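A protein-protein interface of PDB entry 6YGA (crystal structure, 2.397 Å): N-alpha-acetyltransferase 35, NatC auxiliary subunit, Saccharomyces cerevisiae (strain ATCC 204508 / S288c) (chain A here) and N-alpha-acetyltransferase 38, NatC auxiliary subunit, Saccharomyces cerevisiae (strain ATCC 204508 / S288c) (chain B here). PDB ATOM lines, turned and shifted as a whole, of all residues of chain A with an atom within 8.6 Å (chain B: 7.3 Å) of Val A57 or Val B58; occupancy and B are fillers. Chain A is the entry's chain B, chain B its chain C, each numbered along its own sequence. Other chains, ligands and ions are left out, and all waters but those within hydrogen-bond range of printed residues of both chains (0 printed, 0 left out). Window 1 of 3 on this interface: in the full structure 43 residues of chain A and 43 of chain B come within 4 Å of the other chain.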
ATOM      1  N   SER A  54     -22.599  13.136  20.974  1.00  0.00           N
ATOM      2  CA  SER A  54     -21.310  12.472  21.105  1.00  0.00           C
ATOM      3  C   SER A  54     -20.255  13.169  20.259  1.00  0.00           C
ATOM      4  O   SER A  54     -20.547  13.710  19.190  1.00  0.00           O
ATOM      5  CB  SER A  54     -21.397  10.996  20.692  1.00  0.00           C
ATOM      6  OG  SER A  54     -21.807  10.857  19.338  1.00  0.00           O
ATOM      7  N   LEU A  55     -19.021  13.143  20.757  1.00  0.00           N
ATOM      8  CA  LEU A  55     -17.877  13.614  20.001  1.00  0.00           C
ATOM      9  C   LEU A  55     -17.467  12.569  18.964  1.00  0.00           C
ATOM     10  O   LEU A  55     -17.967  11.440  18.947  1.00  0.00           O
ATOM     11  CB  LEU A  55     -16.717  13.927  20.944  1.00  0.00           C
ATOM     12  CG  LEU A  55     -17.026  14.881  22.100  1.00  0.00           C
ATOM     13  CD1 LEU A  55     -15.819  14.991  23.016  1.00  0.00           C
ATOM     14  CD2 LEU A  55     -17.439  16.255  21.586  1.00  0.00           C
ATOM     15  N   GLU A  56     -16.541  12.958  18.088  1.00  0.00           N
ATOM     16  CA  GLU A  56     -16.047  12.062  17.049  1.00  0.00           C
ATOM     17  C   GLU A  56     -14.587  12.376  16.756  1.00  0.00           C
ATOM     18  O   GLU A  56     -14.241  13.529  16.478  1.00  0.00           O
ATOM     19  CB  GLU A  56     -16.884  12.180  15.771  1.00  0.00           C
ATOM     20  CG  GLU A  56     -16.740  10.980  14.856  1.00  0.00           C
ATOM     21  CD  GLU A  56     -17.868  10.865  13.855  1.00  0.00           C
ATOM     22  OE1 GLU A  56     -17.911  11.677  12.907  1.00  0.00           O
ATOM     23  OE2 GLU A  56     -18.720   9.969  14.025  1.00  0.00           O
ATOM     24  N   VAL A  57     -13.740  11.346  16.808  1.00  0.00           N
ATOM     25  CA  VAL A  57     -12.309  11.543  16.616  1.00  0.00           C
ATOM     26  C   VAL A  57     -12.017  11.778  15.140  1.00  0.00           C
ATOM     27  O   VAL A  57     -12.768  11.348  14.255  1.00  0.00           O
ATOM     28  CB  VAL A  57     -11.513  10.339  17.156  1.00  0.00           C
ATOM     29  CG1 VAL A  57     -11.776  10.156  18.642  1.00  0.00           C
ATOM     30  CG2 VAL A  57     -11.868   9.067  16.390  1.00  0.00           C
ATOM     31  N   ASN A  58     -10.922  12.491  14.871  1.00  0.00           N
ATOM     32  CA  ASN A  58     -10.474  12.779  13.508  1.00  0.00           C
ATOM     33  C   ASN A  58     -11.526  13.554  12.712  1.00  0.00           C
ATOM     34  O   ASN A  58     -11.565  13.490  11.480  1.00  0.00           O
ATOM     35  CB  ASN A  58     -10.065  11.492  12.782  1.00  0.00           C
ATOM     36  CG  ASN A  58      -8.848  10.840  13.409  1.00  0.00           C
ATOM     37  OD1 ASN A  58      -7.904  11.522  13.802  1.00  0.00           O
ATOM     38  ND2 ASN A  58      -8.872   9.516  13.524  1.00  0.00           N
ATOM     39  N   ASN A  59     -12.389  14.282  13.419  1.00  0.00           N
ATOM     40  CA  ASN A  59     -13.322  15.237  12.830  1.00  0.00           C
ATOM     41  C   ASN A  59     -12.946  16.602  13.390  1.00  0.00           C
ATOM     42  O   ASN A  59     -13.114  16.848  14.588  1.00  0.00           O
ATOM     43  CB  ASN A  59     -14.771  14.877  13.152  1.00  0.00           C
ATOM     44  CG  ASN A  59     -15.771  15.719  12.380  1.00  0.00           C
ATOM     45  OD1 ASN A  59     -15.557  16.909  12.148  1.00  0.00           O
ATOM     46  ND2 ASN A  59     -16.871  15.099  11.972  1.00  0.00           N
ATOM     47  N   SER A  60     -12.426  17.473  12.523  1.00  0.00           N
ATOM     48  CA  SER A  60     -11.887  18.755  12.971  1.00  0.00           C
ATOM     49  C   SER A  60     -12.890  19.523  13.823  1.00  0.00           C
ATOM     50  O   SER A  60     -12.523  20.120  14.841  1.00  0.00           O
ATOM     51  CB  SER A  60     -11.467  19.591  11.761  1.00  0.00           C
ATOM     52  OG  SER A  60     -10.691  18.822  10.858  1.00  0.00           O
ATOM     53  N   LYS A  61     -14.163  19.502  13.432  1.00  0.00           N
ATOM     54  CA  LYS A  61     -15.182  20.287  14.117  1.00  0.00           C
ATOM     55  C   LYS A  61     -15.720  19.606  15.371  1.00  0.00           C
ATOM     56  O   LYS A  61     -16.399  20.262  16.167  1.00  0.00           O
ATOM     57  CB  LYS A  61     -16.328  20.595  13.147  1.00  0.00           C
ATOM     58  CG  LYS A  61     -15.866  20.990  11.748  1.00  0.00           C
ATOM     59  CD  LYS A  61     -16.904  21.838  11.019  1.00  0.00           C
ATOM     60  CE  LYS A  61     -18.129  21.032  10.612  1.00  0.00           C
ATOM     61  NZ  LYS A  61     -19.193  21.901  10.026  1.00  0.00           N
ATOM     62  N   LEU A  62     -15.419  18.322  15.578  1.00  0.00           N
ATOM     63  CA  LEU A  62     -15.897  17.581  16.742  1.00  0.00           C
ATOM     64  C   LEU A  62     -14.771  16.999  17.592  1.00  0.00           C
ATOM     65  O   LEU A  62     -15.053  16.259  18.544  1.00  0.00           O
ATOM     66  CB  LEU A  62     -16.836  16.451  16.306  1.00  0.00           C
ATOM     67  CG  LEU A  62     -18.266  16.820  15.914  1.00  0.00           C
ATOM     68  CD1 LEU A  62     -18.975  15.625  15.293  1.00  0.00           C
ATOM     69  CD2 LEU A  62     -19.035  17.333  17.120  1.00  0.00           C
ATOM     70  N   ASP A  63     -13.510  17.305  17.287  1.00  0.00           N
ATOM     71  CA  ASP A  63     -12.366  16.740  18.003  1.00  0.00           C
ATOM     72  C   ASP A  63     -11.491  17.885  18.499  1.00  0.00           C
ATOM     73  O   ASP A  63     -10.792  18.525  17.705  1.00  0.00           O
ATOM     74  CB  ASP A  63     -11.569  15.789  17.103  1.00  0.00           C
ATOM     75  CG  ASP A  63     -10.589  14.912  17.877  1.00  0.00           C
ATOM     76  OD1 ASP A  63     -10.202  15.279  19.005  1.00  0.00           O
ATOM     77  OD2 ASP A  63     -10.197  13.849  17.348  1.00  0.00           O
ATOM     78  N   SER A  64     -11.519  18.132  19.813  1.00  0.00           N
ATOM     79  CA  SER A  64     -10.692  19.176  20.409  1.00  0.00           C
ATOM     80  C   SER A  64      -9.217  18.789  20.473  1.00  0.00           C
ATOM     81  O   SER A  64      -8.369  19.660  20.698  1.00  0.00           O
ATOM     82  CB  SER A  64     -11.209  19.520  21.809  1.00  0.00           C
ATOM     83  OG  SER A  64     -11.404  18.354  22.591  1.00  0.00           O
ATOM     84  N   SER A  65      -8.890  17.509  20.285  1.00  0.00           N
ATOM     85  CA  SER A  65      -7.489  17.111  20.240  1.00  0.00           C
ATOM     86  C   SER A  65      -6.796  17.604  18.979  1.00  0.00           C
ATOM     87  O   SER A  65      -5.562  17.625  18.932  1.00  0.00           O
ATOM     88  CB  SER A  65      -7.362  15.590  20.335  1.00  0.00           C
ATOM     89  OG  SER A  65      -7.973  15.099  21.515  1.00  0.00           O
ATOM     90  N   LEU A  66      -7.555  18.006  17.963  1.00  0.00           N
ATOM     91  CA  LEU A  66      -6.983  18.446  16.699  1.00  0.00           C
ATOM     92  C   LEU A  66      -6.929  19.962  16.574  1.00  0.00           C
ATOM     93  O   LEU A  66      -6.677  20.471  15.477  1.00  0.00           O
ATOM     94  CB  LEU A  66      -7.772  17.851  15.532  1.00  0.00           C
ATOM     95  CG  LEU A  66      -7.953  16.332  15.544  1.00  0.00           C
ATOM     96  CD1 LEU A  66      -8.571  15.875  14.236  1.00  0.00           C
ATOM     97  CD2 LEU A  66      -6.637  15.604  15.803  1.00  0.00           C
ATOM     98  N   VAL B  16      -8.568   1.336  22.904  1.00  0.00           N
ATOM     99  CA  VAL B  16      -8.628   1.609  21.472  1.00  0.00           C
ATOM    100  C   VAL B  16      -7.534   2.621  21.152  1.00  0.00           C
ATOM    101  O   VAL B  16      -7.687   3.818  21.422  1.00  0.00           O
ATOM    102  CB  VAL B  16     -10.003   2.125  21.032  1.00  0.00           C
ATOM    103  CG1 VAL B  16      -9.998   2.447  19.544  1.00  0.00           C
ATOM    104  CG2 VAL B  16     -11.078   1.101  21.353  1.00  0.00           C
ATOM    105  N   LEU B  18      -5.673   4.942  18.621  1.00  0.00           N
ATOM    106  CA  LEU B  18      -6.081   5.625  17.403  1.00  0.00           C
ATOM    107  C   LEU B  18      -4.909   5.676  16.423  1.00  0.00           C
ATOM    108  O   LEU B  18      -3.848   5.092  16.656  1.00  0.00           O
ATOM    109  CB  LEU B  18      -6.614   7.017  17.728  1.00  0.00           C
ATOM    110  CG  LEU B  18      -7.874   7.066  18.592  1.00  0.00           C
ATOM    111  CD1 LEU B  18      -8.437   8.478  18.633  1.00  0.00           C
ATOM    112  CD2 LEU B  18      -8.914   6.080  18.083  1.00  0.00           C
ATOM    113  N   ARG B  22      -2.274   8.973  20.349  1.00  0.00           N
ATOM    114  CA  ARG B  22      -3.343   8.984  21.336  1.00  0.00           C
ATOM    115  C   ARG B  22      -3.990   7.608  21.465  1.00  0.00           C
ATOM    116  O   ARG B  22      -4.063   6.833  20.508  1.00  0.00           O
ATOM    117  CB  ARG B  22      -4.395  10.029  20.963  1.00  0.00           C
ATOM    118  CG  ARG B  22      -4.933   9.891  19.548  1.00  0.00           C
ATOM    119  CD  ARG B  22      -5.716  11.124  19.101  1.00  0.00           C
ATOM    120  NE  ARG B  22      -6.931  11.349  19.880  1.00  0.00           N
ATOM    121  CZ  ARG B  22      -7.916  12.155  19.496  1.00  0.00           C
ATOM    122  NH1 ARG B  22      -7.826  12.801  18.341  1.00  0.00           N
ATOM    123  NH2 ARG B  22      -8.990  12.313  20.257  1.00  0.00           N
ATOM    124  N   LEU B  24      -7.501   5.689  23.490  1.00  0.00           N
ATOM    125  CA  LEU B  24      -8.785   5.898  24.146  1.00  0.00           C
ATOM    126  C   LEU B  24      -9.141   4.689  25.001  1.00  0.00           C
ATOM    127  O   LEU B  24      -9.059   3.546  24.537  1.00  0.00           O
ATOM    128  CB  LEU B  24      -9.892   6.156  23.119  1.00  0.00           C
ATOM    129  CG  LEU B  24      -9.679   7.348  22.186  1.00  0.00           C
ATOM    130  CD1 LEU B  24     -10.872   7.523  21.263  1.00  0.00           C
ATOM    131  CD2 LEU B  24      -9.432   8.609  22.992  1.00  0.00           C
ATOM    132  N   LEU B  28     -17.690   0.274  26.197  1.00  0.00           N
ATOM    133  CA  LEU B  28     -18.337   0.120  24.899  1.00  0.00           C
ATOM    134  C   LEU B  28     -19.851   0.242  25.045  1.00  0.00           C
ATOM    135  O   LEU B  28     -20.468  -0.498  25.821  1.00  0.00           O
ATOM    136  CB  LEU B  28     -17.961  -1.223  24.279  1.00  0.00           C
ATOM    137  CG  LEU B  28     -18.522  -1.471  22.879  1.00  0.00           C
ATOM    138  CD1 LEU B  28     -17.890  -0.520  21.875  1.00  0.00           C
ATOM    139  CD2 LEU B  28     -18.323  -2.917  22.460  1.00  0.00           C
ATOM    140  N   ASP B  32     -21.829  -0.993  15.288  1.00  0.00           N
ATOM    141  CA  ASP B  32     -22.679  -1.195  14.123  1.00  0.00           C
ATOM    142  C   ASP B  32     -22.015  -2.167  13.146  1.00  0.00           C
ATOM    143  O   ASP B  32     -20.981  -2.775  13.442  1.00  0.00           O
ATOM    144  CB  ASP B  32     -23.011   0.147  13.459  1.00  0.00           C
ATOM    145  CG  ASP B  32     -21.785   0.853  12.902  1.00  0.00           C
ATOM    146  OD1 ASP B  32     -20.657   0.351  13.088  1.00  0.00           O
ATOM    147  OD2 ASP B  32     -21.959   1.922  12.276  1.00  0.00           O
ATOM    148  N   GLN B  34     -20.478  -1.628  10.344  1.00  0.00           N
ATOM    149  CA  GLN B  34     -19.220  -1.160   9.781  1.00  0.00           C
ATOM    150  C   GLN B  34     -18.135  -0.971  10.839  1.00  0.00           C
ATOM    151  O   GLN B  34     -17.139  -0.289  10.575  1.00  0.00           O
ATOM    152  CB  GLN B  34     -19.448   0.141   9.009  1.00  0.00           C
ATOM    153  CG  GLN B  34     -20.519   0.029   7.926  1.00  0.00           C
ATOM    154  CD  GLN B  34     -20.205  -1.044   6.892  1.00  0.00           C
ATOM    155  OE1 GLN B  34     -21.022  -1.927   6.621  1.00  0.00           O
ATOM    156  NE2 GLN B  34     -19.018  -0.965   6.304  1.00  0.00           N
ATOM    157  N   MET B  35     -18.310  -1.560  12.019  1.00  0.00           N
ATOM    158  CA  MET B  35     -17.351  -1.490  13.123  1.00  0.00           C
ATOM    159  C   MET B  35     -17.126  -0.064  13.630  1.00  0.00           C
ATOM    160  O   MET B  35     -16.060   0.244  14.163  1.00  0.00           O
ATOM    161  CB  MET B  35     -16.010  -2.120  12.725  1.00  0.00           C
ATOM    162  CG  MET B  35     -15.298  -2.822  13.876  1.00  0.00           C
ATOM    163  SD  MET B  35     -13.510  -3.470  13.439  1.00  0.00           S
ATOM    164  CE  MET B  35     -12.557  -1.768  13.419  1.00  0.00           C
ATOM    165  N   ASN B  36     -18.120   0.806  13.464  1.00  0.00           N
ATOM    166  CA  ASN B  36     -18.096   2.087  14.158  1.00  0.00           C
ATOM    167  C   ASN B  36     -18.446   1.858  15.622  1.00  0.00           C
ATOM    168  O   ASN B  36     -19.459   1.224  15.933  1.00  0.00           O
ATOM    169  CB  ASN B  36     -19.080   3.073  13.526  1.00  0.00           C
ATOM    170  CG  ASN B  36     -18.840   3.271  12.042  1.00  0.00           C
ATOM    171  OD1 ASN B  36     -17.698   3.366  11.593  1.00  0.00           O
ATOM    172  ND2 ASN B  36     -19.921   3.327  11.270  1.00  0.00           N
ATOM    173  N   LEU B  37     -17.606   2.355  16.525  1.00  0.00           N
ATOM    174  CA  LEU B  37     -17.797   2.144  17.952  1.00  0.00           C
ATOM    175  C   LEU B  37     -18.246   3.433  18.624  1.00  0.00           C
ATOM    176  O   LEU B  37     -17.840   4.529  18.227  1.00  0.00           O
ATOM    177  CB  LEU B  37     -16.513   1.647  18.620  1.00  0.00           C
ATOM    178  CG  LEU B  37     -15.710   0.561  17.908  1.00  0.00           C
ATOM    179  CD1 LEU B  37     -14.335   0.447  18.534  1.00  0.00           C
ATOM    180  CD2 LEU B  37     -16.437  -0.768  17.969  1.00  0.00           C
ATOM    181  N   LEU B  38     -19.089   3.291  19.642  1.00  0.00           N
ATOM    182  CA  LEU B  38     -19.468   4.390  20.517  1.00  0.00           C
ATOM    183  C   LEU B  38     -19.026   4.038  21.929  1.00  0.00           C
ATOM    184  O   LEU B  38     -19.407   2.988  22.456  1.00  0.00           O
ATOM    185  CB  LEU B  38     -20.978   4.649  20.474  1.00  0.00           C
ATOM    186  CG  LEU B  38     -21.499   5.862  21.251  1.00  0.00           C
ATOM    187  CD1 LEU B  38     -20.955   7.159  20.671  1.00  0.00           C
ATOM    188  CD2 LEU B  38     -23.025   5.875  21.273  1.00  0.00           C
ATOM    189  N   LEU B  39     -18.217   4.905  22.530  1.00  0.00           N
ATOM    190  CA  LEU B  39     -17.618   4.647  23.832  1.00  0.00           C
ATOM    191  C   LEU B  39     -18.019   5.731  24.824  1.00  0.00           C
ATOM    192  O   LEU B  39     -18.096   6.912  24.471  1.00  0.00           O
ATOM    193  CB  LEU B  39     -16.091   4.581  23.728  1.00  0.00           C
ATOM    194  CG  LEU B  39     -15.480   3.507  22.829  1.00  0.00           C
ATOM    195  CD1 LEU B  39     -13.992   3.759  22.646  1.00  0.00           C
ATOM    196  CD2 LEU B  39     -15.717   2.125  23.407  1.00  0.00           C
ATOM    197  N   VAL B  42     -14.864   8.058  28.189  1.00  0.00           N
ATOM    198  CA  VAL B  42     -13.608   7.886  27.467  1.00  0.00           C
ATOM    199  C   VAL B  42     -12.499   8.666  28.156  1.00  0.00           C
ATOM    200  O   VAL B  42     -12.674   9.833  28.531  1.00  0.00           O
ATOM    201  CB  VAL B  42     -13.766   8.328  26.004  1.00  0.00           C
ATOM    202  CG1 VAL B  42     -12.406   8.477  25.335  1.00  0.00           C
ATOM    203  CG2 VAL B  42     -14.611   7.331  25.246  1.00  0.00           C
ATOM    204  N   GLU B  44      -8.686   9.888  27.255  1.00  0.00           N
ATOM    205  CA  GLU B  44      -7.722  10.071  26.177  1.00  0.00           C
ATOM    206  C   GLU B  44      -6.323  10.170  26.772  1.00  0.00           C
ATOM    207  O   GLU B  44      -6.022  11.115  27.508  1.00  0.00           O
ATOM    208  CB  GLU B  44      -8.040  11.322  25.360  1.00  0.00           C
ATOM    209  CG  GLU B  44      -7.234  11.431  24.070  1.00  0.00           C
ATOM    210  CD  GLU B  44      -7.023  12.865  23.626  1.00  0.00           C
ATOM    211  OE1 GLU B  44      -6.790  13.732  24.496  1.00  0.00           O
ATOM    212  OE2 GLU B  44      -7.091  13.128  22.409  1.00  0.00           O
ATOM    213  N   MET B  53     -13.083  12.737  28.131  1.00  0.00           N
ATOM    214  CA  MET B  53     -13.756  13.297  26.962  1.00  0.00           C
ATOM    215  C   MET B  53     -15.221  12.869  26.852  1.00  0.00           C
ATOM    216  O   MET B  53     -15.931  13.300  25.944  1.00  0.00           O
ATOM    217  CB  MET B  53     -13.005  12.911  25.682  1.00  0.00           C
ATOM    218  CG  MET B  53     -11.557  13.380  25.648  1.00  0.00           C
ATOM    219  SD  MET B  53     -10.832  13.468  23.841  1.00  0.00           S
ATOM    220  CE  MET B  53     -11.289  11.672  23.245  1.00  0.00           C
ATOM    221  N   VAL B  56     -17.739   9.362  23.165  1.00  0.00           N
ATOM    222  CA  VAL B  56     -17.032   9.531  21.901  1.00  0.00           C
ATOM    223  C   VAL B  56     -17.375   8.371  20.976  1.00  0.00           C
ATOM    224  O   VAL B  56     -17.492   7.223  21.422  1.00  0.00           O
ATOM    225  CB  VAL B  56     -15.502   9.613  22.110  1.00  0.00           C
ATOM    226  CG1 VAL B  56     -14.820  10.133  20.852  1.00  0.00           C
ATOM    227  CG2 VAL B  56     -15.158  10.483  23.310  1.00  0.00           C
ATOM    228  N   SER B  57     -17.536   8.670  19.690  1.00  0.00           N
ATOM    229  CA  SER B  57     -17.674   7.659  18.652  1.00  0.00           C
ATOM    230  C   SER B  57     -16.400   7.636  17.820  1.00  0.00           C
ATOM    231  O   SER B  57     -15.844   8.689  17.496  1.00  0.00           O
ATOM    232  CB  SER B  57     -18.885   7.936  17.753  1.00  0.00           C
ATOM    233  OG  SER B  57     -18.606   8.953  16.805  1.00  0.00           O
ATOM    234  N   VAL B  58     -15.930   6.439  17.488  1.00  0.00           N
ATOM    235  CA  VAL B  58     -14.711   6.268  16.709  1.00  0.00           C
ATOM    236  C   VAL B  58     -15.071   5.596  15.387  1.00  0.00           C
ATOM    237  O   VAL B  58     -15.629   4.495  15.382  1.00  0.00           O
ATOM    238  CB  VAL B  58     -13.639   5.465  17.468  1.00  0.00           C
ATOM    239  CG1 VAL B  58     -13.118   6.276  18.643  1.00  0.00           C
ATOM    240  CG2 VAL B  58     -14.185   4.140  17.967  1.00  0.00           C
ATOM    241  N   PRO B  59     -14.812   6.232  14.248  1.00  0.00           N
ATOM    242  CA  PRO B  59     -15.110   5.599  12.958  1.00  0.00           C
ATOM    243  C   PRO B  59     -14.152   4.452  12.663  1.00  0.00           C
ATOM    244  O   PRO B  59     -13.189   4.197  13.388  1.00  0.00           O
ATOM    245  CB  PRO B  59     -14.944   6.742  11.950  1.00  0.00           C
ATOM    246  CG  PRO B  59     -15.025   8.003  12.768  1.00  0.00           C
ATOM    247  CD  PRO B  59     -14.436   7.646  14.096  1.00  0.00           C
ATOM    248  N   ARG B  60     -14.437   3.757  11.560  1.00  0.00           N
ATOM    249  CA  ARG B  60     -13.648   2.588  11.182  1.00  0.00           C
ATOM    250  C   ARG B  60     -12.194   2.958  10.908  1.00  0.00           C
ATOM    251  O   ARG B  60     -11.271   2.333  11.442  1.00  0.00           O
ATOM    252  CB  ARG B  60     -14.270   1.920   9.955  1.00  0.00           C
ATOM    253  CG  ARG B  60     -13.316   1.015   9.198  1.00  0.00           C
ATOM    254  CD  ARG B  60     -13.900   0.566   7.868  1.00  0.00           C
ATOM    255  NE  ARG B  60     -12.960  -0.274   7.131  1.00  0.00           N
ATOM    256  CZ  ARG B  60     -12.808  -1.578   7.339  1.00  0.00           C
ATOM    257  NH1 ARG B  60     -13.534  -2.192   8.263  1.00  0.00           N
ATOM    258  NH2 ARG B  60     -11.929  -2.269   6.628  1.00  0.00           N
ATOM    259  N   ARG B  61     -11.975   3.975  10.070  1.00  0.00           N
ATOM    260  CA  ARG B  61     -10.619   4.339   9.671  1.00  0.00           C
ATOM    261  C   ARG B  61      -9.762   4.740  10.865  1.00  0.00           C
ATOM    262  O   ARG B  61      -8.540   4.561  10.841  1.00  0.00           O
ATOM    263  CB  ARG B  61     -10.667   5.477   8.651  1.00  0.00           C
ATOM    264  CG  ARG B  61      -9.322   5.840   8.041  1.00  0.00           C
ATOM    265  CD  ARG B  61      -9.277   7.303   7.621  1.00  0.00           C
ATOM    266  NE  ARG B  61      -9.202   8.201   8.771  1.00  0.00           N
ATOM    267  CZ  ARG B  61      -9.057   9.520   8.681  1.00  0.00           C
ATOM    268  NH1 ARG B  61      -8.972  10.099   7.492  1.00  0.00           N
ATOM    269  NH2 ARG B  61      -8.997  10.261   9.780  1.00  0.00           N
ATOM    270  N   SER B  62     -10.381   5.267  11.919  1.00  0.00           N
ATOM    271  CA  SER B  62      -9.628   5.841  13.026  1.00  0.00           C
ATOM    272  C   SER B  62      -9.077   4.800  13.991  1.00  0.00           C
ATOM    273  O   SER B  62      -8.131   5.101  14.728  1.00  0.00           O
ATOM    274  CB  SER B  62     -10.508   6.829  13.790  1.00  0.00           C
ATOM    275  OG  SER B  62     -10.837   7.938  12.970  1.00  0.00           O
ATOM    276  N   VAL B  63      -9.634   3.596  14.009  1.00  0.00           N
ATOM    277  CA  VAL B  63      -9.270   2.594  15.001  1.00  0.00           C
ATOM    278  C   VAL B  63      -8.048   1.824  14.514  1.00  0.00           C
ATOM    279  O   VAL B  63      -8.093   1.166  13.469  1.00  0.00           O
ATOM    280  CB  VAL B  63     -10.444   1.646  15.284  1.00  0.00           C
ATOM    281  CG1 VAL B  63      -9.997   0.477  16.142  1.00  0.00           C
ATOM    282  CG2 VAL B  63     -11.573   2.405  15.962  1.00  0.00           C
ATOM    283  N   ILE B  66      -8.078  -2.792  18.927  1.00  0.00           N
ATOM    284  CA  ILE B  66      -9.017  -2.918  20.034  1.00  0.00           C
ATOM    285  C   ILE B  66      -8.473  -3.965  20.994  1.00  0.00           C
ATOM    286  O   ILE B  66      -8.164  -5.090  20.583  1.00  0.00           O
ATOM    287  CB  ILE B  66     -10.426  -3.299  19.542  1.00  0.00           C
ATOM    288  CG1 ILE B  66     -10.953  -2.247  18.565  1.00  0.00           C
ATOM    289  CG2 ILE B  66     -11.384  -3.441  20.713  1.00  0.00           C
ATOM    290  CD1 ILE B  66     -12.284  -2.606  17.942  1.00  0.00           C
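Val A57 touches just these residues of chain B: Leu B18, Arg B22, Leu B24, Val B56, Ser B57, Val B58, Pro B59 and Ser B62. Val B58 touches just one residue of chain A: Val A57. Of chain A, only Leu A55 (2.9 Å), Glu A56 (3.0 Å) and Val A57 (3.5 Å) come within 4 Å of Ser B57. Of the printed residues of chain A, Ser B62 touches Val A57 and Asn A58. Printed residues of chain B within 4 Å of Asp A63: Arg B22. Of the printed residues of chain A, Leu B18 touches Val A57. The nearest printed residue of chain A that does not touch Val B56 is Glu A56 (4.3 Å).
OG of Ser A65 sits close to OE1 of Glu B44. The side-chain carboxylate (OD2) of Asp A63 is in salt-bridge range of the guanidinium group (NH1) of Arg B22. The guanidinium group (NH2) of Arg B22 sits at hydrogen-bond distance from the side-chain hydroxyl (OG) of Ser A65 (3.2 Å). ND2 of Asn A58 lies within hydrogen-bond range of OG of Ser B62 (2.6 Å). The backbone NH (N) of Val A57 lies within hydrogen-bond range of the backbone carbonyl oxygen (O) of Ser B57 (3.5 Å). N of Ser B57 lies within hydrogen-bond range of O of Leu A55 (2.9 Å). The side-chain hydroxyl of Ser B57 sits at hydrogen-bond distance from the side-chain carboxylate of Glu A56 (3.0 Å).
Of the 24 printed residues of chain B, 12 touch a printed residue of chain A. Of the 13 printed residues of chain A, 8 touch a printed residue of chain B. Among the printed residues, 19 pairs touch across the chains.
The side-chain carboxylate of Asp A63 is in hydrogen-bond range of the backbone NH of Ser A65. N of Leu B39 lies within hydrogen-bond range of O of Val B56 (2.7 Å). N of Asn A58 is in hydrogen-bond range of OD2 of Asp A63 (2.9 Å). The backbone carbonyl oxygen (O) of Val B42 is in hydrogen-bond range of the backbone NH (N) of Met B53. The backbone NH (N) of Val B16 is in hydrogen-bond range of the backbone carbonyl oxygen (O) of Leu B24 (2.8 Å). The guanidinium group (NH2) of Arg B22 is in salt-bridge range of the side-chain carboxylate (OE2) of Glu B44, 3.0 Å away.
CB of Ser A54 touches CD1 of Leu B38, at 3.9 Å. Leu A55 touches Met B53. Val B56 touches Leu A55 (CA to O, 3.6 Å). Leu B18 touches Val A57 (CD1 to CG1, 3.7 Å). CG1 of Val A57 touches NH2 of Arg B22 (3.9 Å). Leu B24 touches Val A57. CG1 of Val A57 touches CG1 of Val B56 (3.8 Å). Val A57 touches Ser B62 (CG2 to CB, 3.7 Å). Arg B61 touches Asn A58. Leu A66 touches Arg B22 (CD2 to NH1, 3.96 Å).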
